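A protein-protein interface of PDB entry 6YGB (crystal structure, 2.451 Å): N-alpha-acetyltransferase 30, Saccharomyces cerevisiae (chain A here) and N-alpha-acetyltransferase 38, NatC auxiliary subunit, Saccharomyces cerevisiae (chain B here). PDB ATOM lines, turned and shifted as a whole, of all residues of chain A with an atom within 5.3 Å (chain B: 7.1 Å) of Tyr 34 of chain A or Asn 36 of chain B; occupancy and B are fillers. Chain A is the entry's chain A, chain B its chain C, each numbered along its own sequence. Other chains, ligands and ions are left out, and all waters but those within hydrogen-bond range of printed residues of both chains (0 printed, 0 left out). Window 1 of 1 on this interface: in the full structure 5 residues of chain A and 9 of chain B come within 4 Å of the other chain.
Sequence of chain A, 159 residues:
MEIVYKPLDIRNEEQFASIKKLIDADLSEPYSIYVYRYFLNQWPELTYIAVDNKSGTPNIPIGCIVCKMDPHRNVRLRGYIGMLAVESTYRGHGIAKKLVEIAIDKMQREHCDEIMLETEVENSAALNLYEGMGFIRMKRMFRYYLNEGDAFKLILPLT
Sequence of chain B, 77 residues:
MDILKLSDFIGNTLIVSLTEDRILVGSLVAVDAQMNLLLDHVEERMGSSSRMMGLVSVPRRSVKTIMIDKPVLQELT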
ATOM      1  N   SER A  32       9.815 -15.207 -11.439  1.00  0.00           N
ATOM      2  CA  SER A  32       9.362 -16.210 -10.491  1.00  0.00           C
ATOM      3  C   SER A  32      10.523 -16.636  -9.597  1.00  0.00           C
ATOM      4  O   SER A  32      11.687 -16.317  -9.851  1.00  0.00           O
ATOM      5  CB  SER A  32       8.775 -17.423 -11.214  1.00  0.00           C
ATOM      6  OG  SER A  32       9.796 -18.280 -11.701  1.00  0.00           O
ATOM      7  N   ILE A  33      10.189 -17.368  -8.529  1.00  0.00           N
ATOM      8  CA  ILE A  33      11.212 -17.854  -7.603  1.00  0.00           C
ATOM      9  C   ILE A  33      12.251 -18.685  -8.341  1.00  0.00           C
ATOM     10  O   ILE A  33      13.451 -18.617  -8.048  1.00  0.00           O
ATOM     11  CB  ILE A  33      10.563 -18.654  -6.457  1.00  0.00           C
ATOM     12  CG1 ILE A  33       9.835 -17.714  -5.493  1.00  0.00           C
ATOM     13  CG2 ILE A  33      11.602 -19.497  -5.724  1.00  0.00           C
ATOM     14  CD1 ILE A  33       9.019 -18.429  -4.437  1.00  0.00           C
ATOM     15  N   TYR A  34      11.812 -19.469  -9.323  1.00  0.00           N
ATOM     16  CA  TYR A  34      12.736 -20.350 -10.023  1.00  0.00           C
ATOM     17  C   TYR A  34      13.581 -19.623 -11.058  1.00  0.00           C
ATOM     18  O   TYR A  34      14.562 -20.194 -11.547  1.00  0.00           O
ATOM     19  CB  TYR A  34      11.976 -21.509 -10.662  1.00  0.00           C
ATOM     20  CG  TYR A  34      11.845 -22.669  -9.713  1.00  0.00           C
ATOM     21  CD1 TYR A  34      10.769 -22.757  -8.838  1.00  0.00           C
ATOM     22  CD2 TYR A  34      12.815 -23.659  -9.665  1.00  0.00           C
ATOM     23  CE1 TYR A  34      10.656 -23.810  -7.957  1.00  0.00           C
ATOM     24  CE2 TYR A  34      12.709 -24.716  -8.789  1.00  0.00           C
ATOM     25  CZ  TYR A  34      11.626 -24.785  -7.935  1.00  0.00           C
ATOM     26  OH  TYR A  34      11.516 -25.835  -7.059  1.00  0.00           O
ATOM     27  N   VAL A  35      13.230 -18.384 -11.405  1.00  0.00           N
ATOM     28  CA  VAL A  35      14.186 -17.525 -12.098  1.00  0.00           C
ATOM     29  C   VAL A  35      15.349 -17.209 -11.172  1.00  0.00           C
ATOM     30  O   VAL A  35      16.520 -17.275 -11.561  1.00  0.00           O
ATOM     31  CB  VAL A  35      13.505 -16.237 -12.594  1.00  0.00           C
ATOM     32  CG1 VAL A  35      14.531 -15.322 -13.242  1.00  0.00           C
ATOM     33  CG2 VAL A  35      12.379 -16.553 -13.557  1.00  0.00           C
ATOM     34  N   TYR A  36      15.034 -16.869  -9.922  1.00  0.00           N
ATOM     35  CA  TYR A  36      16.065 -16.571  -8.936  1.00  0.00           C
ATOM     36  C   TYR A  36      16.833 -17.829  -8.542  1.00  0.00           C
ATOM     37  O   TYR A  36      18.046 -17.773  -8.313  1.00  0.00           O
ATOM     38  CB  TYR A  36      15.434 -15.910  -7.707  1.00  0.00           C
ATOM     39  CG  TYR A  36      14.910 -14.510  -7.959  1.00  0.00           C
ATOM     40  CD1 TYR A  36      15.768 -13.418  -7.959  1.00  0.00           C
ATOM     41  CD2 TYR A  36      13.558 -14.279  -8.187  1.00  0.00           C
ATOM     42  CE1 TYR A  36      15.299 -12.139  -8.184  1.00  0.00           C
ATOM     43  CE2 TYR A  36      13.080 -13.001  -8.415  1.00  0.00           C
ATOM     44  CZ  TYR A  36      13.957 -11.935  -8.413  1.00  0.00           C
ATOM     45  OH  TYR A  36      13.496 -10.659  -8.639  1.00  0.00           O
ATOM     46  N   ARG A  37      16.144 -18.972  -8.454  1.00  0.00           N
ATOM     47  CA  ARG A  37      16.817 -20.224  -8.115  1.00  0.00           C
ATOM     48  C   ARG A  37      17.847 -20.599  -9.169  1.00  0.00           C
ATOM     49  O   ARG A  37      18.932 -21.093  -8.840  1.00  0.00           O
ATOM     50  CB  ARG A  37      15.796 -21.355  -7.958  1.00  0.00           C
ATOM     51  CG  ARG A  37      15.029 -21.344  -6.647  1.00  0.00           C
ATOM     52  CD  ARG A  37      15.941 -21.660  -5.480  1.00  0.00           C
ATOM     53  NE  ARG A  37      15.324 -21.338  -4.198  1.00  0.00           N
ATOM     54  CZ  ARG A  37      15.975 -21.350  -3.041  1.00  0.00           C
ATOM     55  NH1 ARG A  37      17.261 -21.670  -3.012  1.00  0.00           N
ATOM     56  NH2 ARG A  37      15.344 -21.043  -1.914  1.00  0.00           N
ATOM     57  N   TYR A  38      17.516 -20.377 -10.443  1.00  0.00           N
ATOM     58  CA  TYR A  38      18.426 -20.728 -11.531  1.00  0.00           C
ATOM     59  C   TYR A  38      19.765 -20.015 -11.392  1.00  0.00           C
ATOM     60  O   TYR A  38      20.821 -20.621 -11.601  1.00  0.00           O
ATOM     61  CB  TYR A  38      17.772 -20.402 -12.875  1.00  0.00           C
ATOM     62  CG  TYR A  38      18.741 -20.257 -14.029  1.00  0.00           C
ATOM     63  CD1 TYR A  38      19.293 -21.373 -14.643  1.00  0.00           C
ATOM     64  CD2 TYR A  38      19.089 -19.002 -14.513  1.00  0.00           C
ATOM     65  CE1 TYR A  38      20.173 -21.245 -15.698  1.00  0.00           C
ATOM     66  CE2 TYR A  38      19.967 -18.863 -15.569  1.00  0.00           C
ATOM     67  CZ  TYR A  38      20.507 -19.987 -16.158  1.00  0.00           C
ATOM     68  OH  TYR A  38      21.383 -19.851 -17.212  1.00  0.00           O
ATOM     69  N   LEU B  28       5.673 -32.889 -11.648  1.00  0.00           N
ATOM     70  CA  LEU B  28       6.650 -32.249 -10.766  1.00  0.00           C
ATOM     71  C   LEU B  28       8.007 -32.155 -11.459  1.00  0.00           C
ATOM     72  O   LEU B  28       8.669 -33.176 -11.687  1.00  0.00           O
ATOM     73  CB  LEU B  28       6.756 -33.014  -9.449  1.00  0.00           C
ATOM     74  CG  LEU B  28       7.736 -32.401  -8.447  1.00  0.00           C
ATOM     75  CD1 LEU B  28       7.172 -31.118  -7.860  1.00  0.00           C
ATOM     76  CD2 LEU B  28       8.065 -33.394  -7.355  1.00  0.00           C
ATOM     77  N   VAL B  29       8.425 -30.924 -11.774  1.00  0.00           N
ATOM     78  CA  VAL B  29       9.708 -30.702 -12.437  1.00  0.00           C
ATOM     79  C   VAL B  29      10.836 -30.588 -11.422  1.00  0.00           C
ATOM     80  O   VAL B  29      11.906 -31.182 -11.598  1.00  0.00           O
ATOM     81  CB  VAL B  29       9.642 -29.453 -13.328  1.00  0.00           C
ATOM     82  CG1 VAL B  29      11.047 -28.969 -13.651  1.00  0.00           C
ATOM     83  CG2 VAL B  29       8.890 -29.750 -14.603  1.00  0.00           C
ATOM     84  N   ALA B  30      10.632 -29.807 -10.363  1.00  0.00           N
ATOM     85  CA  ALA B  30      11.669 -29.626  -9.357  1.00  0.00           C
ATOM     86  C   ALA B  30      11.046 -29.182  -8.041  1.00  0.00           C
ATOM     87  O   ALA B  30       9.921 -28.677  -7.999  1.00  0.00           O
ATOM     88  CB  ALA B  30      12.724 -28.613  -9.815  1.00  0.00           C
ATOM     89  N   VAL B  31      11.800 -29.385  -6.964  1.00  0.00           N
ATOM     90  CA  VAL B  31      11.434 -28.924  -5.630  1.00  0.00           C
ATOM     91  C   VAL B  31      12.712 -28.466  -4.943  1.00  0.00           C
ATOM     92  O   VAL B  31      13.776 -29.062  -5.138  1.00  0.00           O
ATOM     93  CB  VAL B  31      10.715 -30.026  -4.817  1.00  0.00           C
ATOM     94  CG1 VAL B  31      11.606 -31.253  -4.648  1.00  0.00           C
ATOM     95  CG2 VAL B  31      10.256 -29.491  -3.466  1.00  0.00           C
ATOM     96  N   ASP B  32      12.620 -27.391  -4.160  1.00  0.00           N
ATOM     97  CA  ASP B  32      13.787 -26.816  -3.500  1.00  0.00           C
ATOM     98  C   ASP B  32      13.713 -27.036  -1.988  1.00  0.00           C
ATOM     99  O   ASP B  32      12.813 -27.704  -1.472  1.00  0.00           O
ATOM    100  CB  ASP B  32      13.933 -25.331  -3.848  1.00  0.00           C
ATOM    101  CG  ASP B  32      12.851 -24.466  -3.230  1.00  0.00           C
ATOM    102  OD1 ASP B  32      11.919 -25.007  -2.599  1.00  0.00           O
ATOM    103  OD2 ASP B  32      12.939 -23.228  -3.377  1.00  0.00           O
ATOM    104  N   ALA B  33      14.676 -26.442  -1.276  1.00  0.00           N
ATOM    105  CA  ALA B  33      14.805 -26.678   0.161  1.00  0.00           C
ATOM    106  C   ALA B  33      13.650 -26.084   0.954  1.00  0.00           C
ATOM    107  O   ALA B  33      13.304 -26.605   2.021  1.00  0.00           O
ATOM    108  CB  ALA B  33      16.127 -26.112   0.670  1.00  0.00           C
ATOM    109  N   GLN B  34      13.056 -24.996   0.470  1.00  0.00           N
ATOM    110  CA  GLN B  34      11.925 -24.371   1.135  1.00  0.00           C
ATOM    111  C   GLN B  34      10.589 -24.864   0.592  1.00  0.00           C
ATOM    112  O   GLN B  34       9.571 -24.179   0.748  1.00  0.00           O
ATOM    113  CB  GLN B  34      12.022 -22.851   1.013  1.00  0.00           C
ATOM    114  CG  GLN B  34      13.381 -22.292   1.406  1.00  0.00           C
ATOM    115  CD  GLN B  34      13.744 -22.588   2.851  1.00  0.00           C
ATOM    116  OE1 GLN B  34      14.890 -22.916   3.161  1.00  0.00           O
ATOM    117  NE2 GLN B  34      12.767 -22.468   3.745  1.00  0.00           N
ATOM    118  N   MET B  35      10.584 -26.032  -0.054  1.00  0.00           N
ATOM    119  CA  MET B  35       9.388 -26.676  -0.599  1.00  0.00           C
ATOM    120  C   MET B  35       8.679 -25.809  -1.640  1.00  0.00           C
ATOM    121  O   MET B  35       7.465 -25.917  -1.824  1.00  0.00           O
ATOM    122  CB  MET B  35       8.414 -27.084   0.513  1.00  0.00           C
ATOM    123  CG  MET B  35       7.541 -28.282   0.152  1.00  0.00           C
ATOM    124  SD  MET B  35       6.409 -28.771   1.469  1.00  0.00           S
ATOM    125  CE  MET B  35       5.373 -27.314   1.574  1.00  0.00           C
ATOM    126  N   ASN B  36       9.422 -24.942  -2.329  1.00  0.00           N
ATOM    127  CA  ASN B  36       8.889 -24.290  -3.519  1.00  0.00           C
ATOM    128  C   ASN B  36       8.852 -25.303  -4.651  1.00  0.00           C
ATOM    129  O   ASN B  36       9.840 -26.002  -4.897  1.00  0.00           O
ATOM    130  CB  ASN B  36       9.748 -23.088  -3.918  1.00  0.00           C
ATOM    131  CG  ASN B  36       9.865 -22.056  -2.816  1.00  0.00           C
ATOM    132  OD1 ASN B  36       8.895 -21.764  -2.119  1.00  0.00           O
ATOM    133  ND2 ASN B  36      11.063 -21.498  -2.652  1.00  0.00           N
ATOM    134  N   LEU B  37       7.716 -25.397  -5.332  1.00  0.00           N
ATOM    135  CA  LEU B  37       7.510 -26.401  -6.364  1.00  0.00           C
ATOM    136  C   LEU B  37       7.518 -25.759  -7.742  1.00  0.00           C
ATOM    137  O   LEU B  37       7.093 -24.615  -7.916  1.00  0.00           O
ATOM    138  CB  LEU B  37       6.184 -27.136  -6.158  1.00  0.00           C
ATOM    139  CG  LEU B  37       5.914 -27.782  -4.800  1.00  0.00           C
ATOM    140  CD1 LEU B  37       4.447 -28.120  -4.687  1.00  0.00           C
ATOM    141  CD2 LEU B  37       6.764 -29.027  -4.604  1.00  0.00           C
ATOM    142  N   LEU B  38       8.009 -26.508  -8.726  1.00  0.00           N
ATOM    143  CA  LEU B  38       7.900 -26.138 -10.130  1.00  0.00           C
ATOM    144  C   LEU B  38       7.180 -27.272 -10.838  1.00  0.00           C
ATOM    145  O   LEU B  38       7.646 -28.417 -10.812  1.00  0.00           O
ATOM    146  CB  LEU B  38       9.272 -25.881 -10.758  1.00  0.00           C
ATOM    147  CG  LEU B  38       9.278 -25.332 -12.190  1.00  0.00           C
ATOM    148  CD1 LEU B  38       8.626 -23.957 -12.258  1.00  0.00           C
ATOM    149  CD2 LEU B  38      10.695 -25.280 -12.740  1.00  0.00           C
ATOM    150  N   LEU B  39       6.042 -26.961 -11.451  1.00  0.00           N
ATOM    151  CA  LEU B  39       5.191 -27.956 -12.083  1.00  0.00           C
ATOM    152  C   LEU B  39       5.050 -27.666 -13.570  1.00  0.00           C
ATOM    153  O   LEU B  39       5.001 -26.504 -13.987  1.00  0.00           O
ATOM    154  CB  LEU B  39       3.806 -27.991 -11.428  1.00  0.00           C
ATOM    155  CG  LEU B  39       3.697 -28.421  -9.964  1.00  0.00           C
ATOM    156  CD1 LEU B  39       2.269 -28.254  -9.466  1.00  0.00           C
ATOM    157  CD2 LEU B  39       4.157 -29.856  -9.793  1.00  0.00           C
ATOM    158  N   VAL B  56       4.426 -23.783 -14.254  1.00  0.00           N
ATOM    159  CA  VAL B  56       4.025 -22.947 -13.132  1.00  0.00           C
ATOM    160  C   VAL B  56       4.900 -23.267 -11.934  1.00  0.00           C
ATOM    161  O   VAL B  56       5.218 -24.432 -11.676  1.00  0.00           O
ATOM    162  CB  VAL B  56       2.541 -23.143 -12.766  1.00  0.00           C
ATOM    163  CG1 VAL B  56       2.074 -22.006 -11.870  1.00  0.00           C
ATOM    164  CG2 VAL B  56       1.687 -23.242 -14.014  1.00  0.00           C
ATOM    165  N   SER B  57       5.282 -22.233 -11.200  1.00  0.00           N
ATOM    166  CA  SER B  57       5.992 -22.379  -9.944  1.00  0.00           C
ATOM    167  C   SER B  57       5.024 -22.059  -8.816  1.00  0.00           C
ATOM    168  O   SER B  57       4.281 -21.076  -8.888  1.00  0.00           O
ATOM    169  CB  SER B  57       7.210 -21.460  -9.886  1.00  0.00           C
ATOM    170  OG  SER B  57       6.819 -20.099  -9.873  1.00  0.00           O
ATOM    171  N   VAL B  58       5.029 -22.893  -7.786  1.00  0.00           N
ATOM    172  CA  VAL B  58       4.105 -22.795  -6.665  1.00  0.00           C
ATOM    173  C   VAL B  58       4.916 -22.558  -5.397  1.00  0.00           C
ATOM    174  O   VAL B  58       5.647 -23.451  -4.954  1.00  0.00           O
ATOM    175  CB  VAL B  58       3.241 -24.059  -6.521  1.00  0.00           C
ATOM    176  CG1 VAL B  58       2.106 -23.810  -5.559  1.00  0.00           C
ATOM    177  CG2 VAL B  58       2.723 -24.499  -7.881  1.00  0.00           C
ATOM    178  N   PRO B  59       4.821 -21.384  -4.773  1.00  0.00           N
ATOM    179  CA  PRO B  59       5.569 -21.130  -3.535  1.00  0.00           C
ATOM    180  C   PRO B  59       4.993 -21.921  -2.368  1.00  0.00           C
ATOM    181  O   PRO B  59       3.878 -22.443  -2.418  1.00  0.00           O
ATOM    182  CB  PRO B  59       5.404 -19.621  -3.317  1.00  0.00           C
ATOM    183  CG  PRO B  59       4.954 -19.081  -4.637  1.00  0.00           C
ATOM    184  CD  PRO B  59       4.166 -20.171  -5.285  1.00  0.00           C
ATOM    185  N   ARG B  60       5.785 -21.995  -1.295  1.00  0.00           N
ATOM    186  CA  ARG B  60       5.440 -22.834  -0.148  1.00  0.00           C
ATOM    187  C   ARG B  60       4.134 -22.392   0.508  1.00  0.00           C
ATOM    188  O   ARG B  60       3.257 -23.218   0.789  1.00  0.00           O
ATOM    189  CB  ARG B  60       6.587 -22.804   0.864  1.00  0.00           C
ATOM    190  CG  ARG B  60       6.267 -23.474   2.182  1.00  0.00           C
ATOM    191  CD  ARG B  60       7.299 -23.132   3.245  1.00  0.00           C
ATOM    192  NE  ARG B  60       6.851 -23.510   4.584  1.00  0.00           N
ATOM    193  CZ  ARG B  60       7.107 -24.683   5.157  1.00  0.00           C
ATOM    194  NH1 ARG B  60       7.815 -25.598   4.506  1.00  0.00           N
ATOM    195  NH2 ARG B  60       6.661 -24.940   6.381  1.00  0.00           N
ATOM    196  N   ARG B  61       4.000 -21.090   0.776  1.00  0.00           N
ATOM    197  CA  ARG B  61       2.800 -20.571   1.428  1.00  0.00           C
ATOM    198  C   ARG B  61       1.546 -20.876   0.621  1.00  0.00           C
ATOM    199  O   ARG B  61       0.479 -21.122   1.196  1.00  0.00           O
ATOM    200  CB  ARG B  61       2.926 -19.059   1.629  1.00  0.00           C
ATOM    201  CG  ARG B  61       1.718 -18.424   2.299  1.00  0.00           C
ATOM    202  CD  ARG B  61       1.463 -16.999   1.818  1.00  0.00           C
ATOM    203  NE  ARG B  61       0.783 -16.956   0.524  1.00  0.00           N
ATOM    204  CZ  ARG B  61       0.139 -15.892   0.054  1.00  0.00           C
ATOM    205  NH1 ARG B  61       0.079 -14.780   0.773  1.00  0.00           N
ATOM    206  NH2 ARG B  61      -0.452 -15.942  -1.133  1.00  0.00           N
ATOM    207  N   VAL B  63       0.789 -23.444  -1.182  1.00  0.00           N
ATOM    208  CA  VAL B  63       0.394 -24.849  -1.233  1.00  0.00           C
ATOM    209  C   VAL B  63      -0.503 -25.155  -0.038  1.00  0.00           C
ATOM    210  O   VAL B  63      -0.065 -25.091   1.114  1.00  0.00           O
ATOM    211  CB  VAL B  63       1.611 -25.781  -1.249  1.00  0.00           C
ATOM    212  CG1 VAL B  63       1.165 -27.222  -1.059  1.00  0.00           C
ATOM    213  CG2 VAL B  63       2.384 -25.635  -2.550  1.00  0.00           C
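The backbone carbonyl oxygen of Ala 30 of chain B sits at hydrogen-bond distance from the side-chain hydroxyl of Tyr 34 of chain A, 3.4 Å away.
OH of Tyr 34 of chain A lies within hydrogen-bond range of N of Asp 32 of chain B (3.5 Å).
The side-chain hydroxyl (OH) of Tyr 34 of chain A sits at hydrogen-bond distance from the backbone carbonyl oxygen (O) of Asn 36 of chain B (2.7 Å).
NE of Arg 37 of chain A is in salt-bridge range of OD2 of Asp 32 of chain B.
OG of Ser 32 of chain A lies close to N of Tyr 34 of chain A, 3.3 Å away.
The side-chain hydroxyl (OG) of Ser 32 of chain A sits at hydrogen-bond distance from the backbone NH (N) of Val 35 of chain A (3.4 Å).
O of Ala 30 of chain B lies within hydrogen-bond range of N of Leu 38 of chain B, 3.0 Å away.
N of Gln 34 of chain B sits close to OD1 of Asp 32 of chain B, at 3.3 Å.
The backbone NH (N) of Arg 60 of chain B lies within hydrogen-bond range of the side-chain amide oxygen (OD1) of Asn 36 of chain B (3.2 Å).
O of Leu 37 of chain B is in hydrogen-bond range of N of Val 58 of chain B, at 2.7 Å.
Among the printed residues, merely in contact across the chains: Tyr 34 of chain A with Val 31 of chain B (3.4 Å), Ser 32 of chain A with Ser 57 of chain B (3.6 Å), Tyr 34 of chain A with Leu 37 of chain B (3.7 Å), Ile 33 of chain A with Asn 36 of chain B (3.7 Å), Tyr 34 of chain A with Leu 38 of chain B (3.7 Å), Tyr 34 of chain A with Ser 57 of chain B (3.9 Å) and Ile 33 of chain A with Pro 59 of chain B (3.97 Å).
Val 35 of chain A touches none of the printed residues of chain B.
Of the printed residues of chain A, Ala 30 of chain B touches Tyr 34.
Asn 36 of chain B touches just these residues of chain A: Ile 33 and Tyr 34.
Of the printed residues of chain A, Leu 38 of chain B touches Tyr 34.
The nearest residue of chain A that does not touch Asn 36 of chain B is Arg 37 of chain A (4.4 Å).
The nearest printed residue of chain A that does not touch Leu 38 of chain B is Ser 32 of chain A (5.8 Å).
Of the 7 printed residues of chain A, 4 touch a printed residue of chain B.
Hydrophobic or aromatic side chains of chain A within 4 Å of the printed part of chain B: Ile 33 and Tyr 34.
Of the 19 printed residues of chain B, 8 touch a printed residue of chain A.
Hydrophobic or aromatic side chains of chain B within 4 Å of the printed part of chain A: Leu 38 and Pro 59.
Among the printed residues, 11 pairs touch across the chains.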
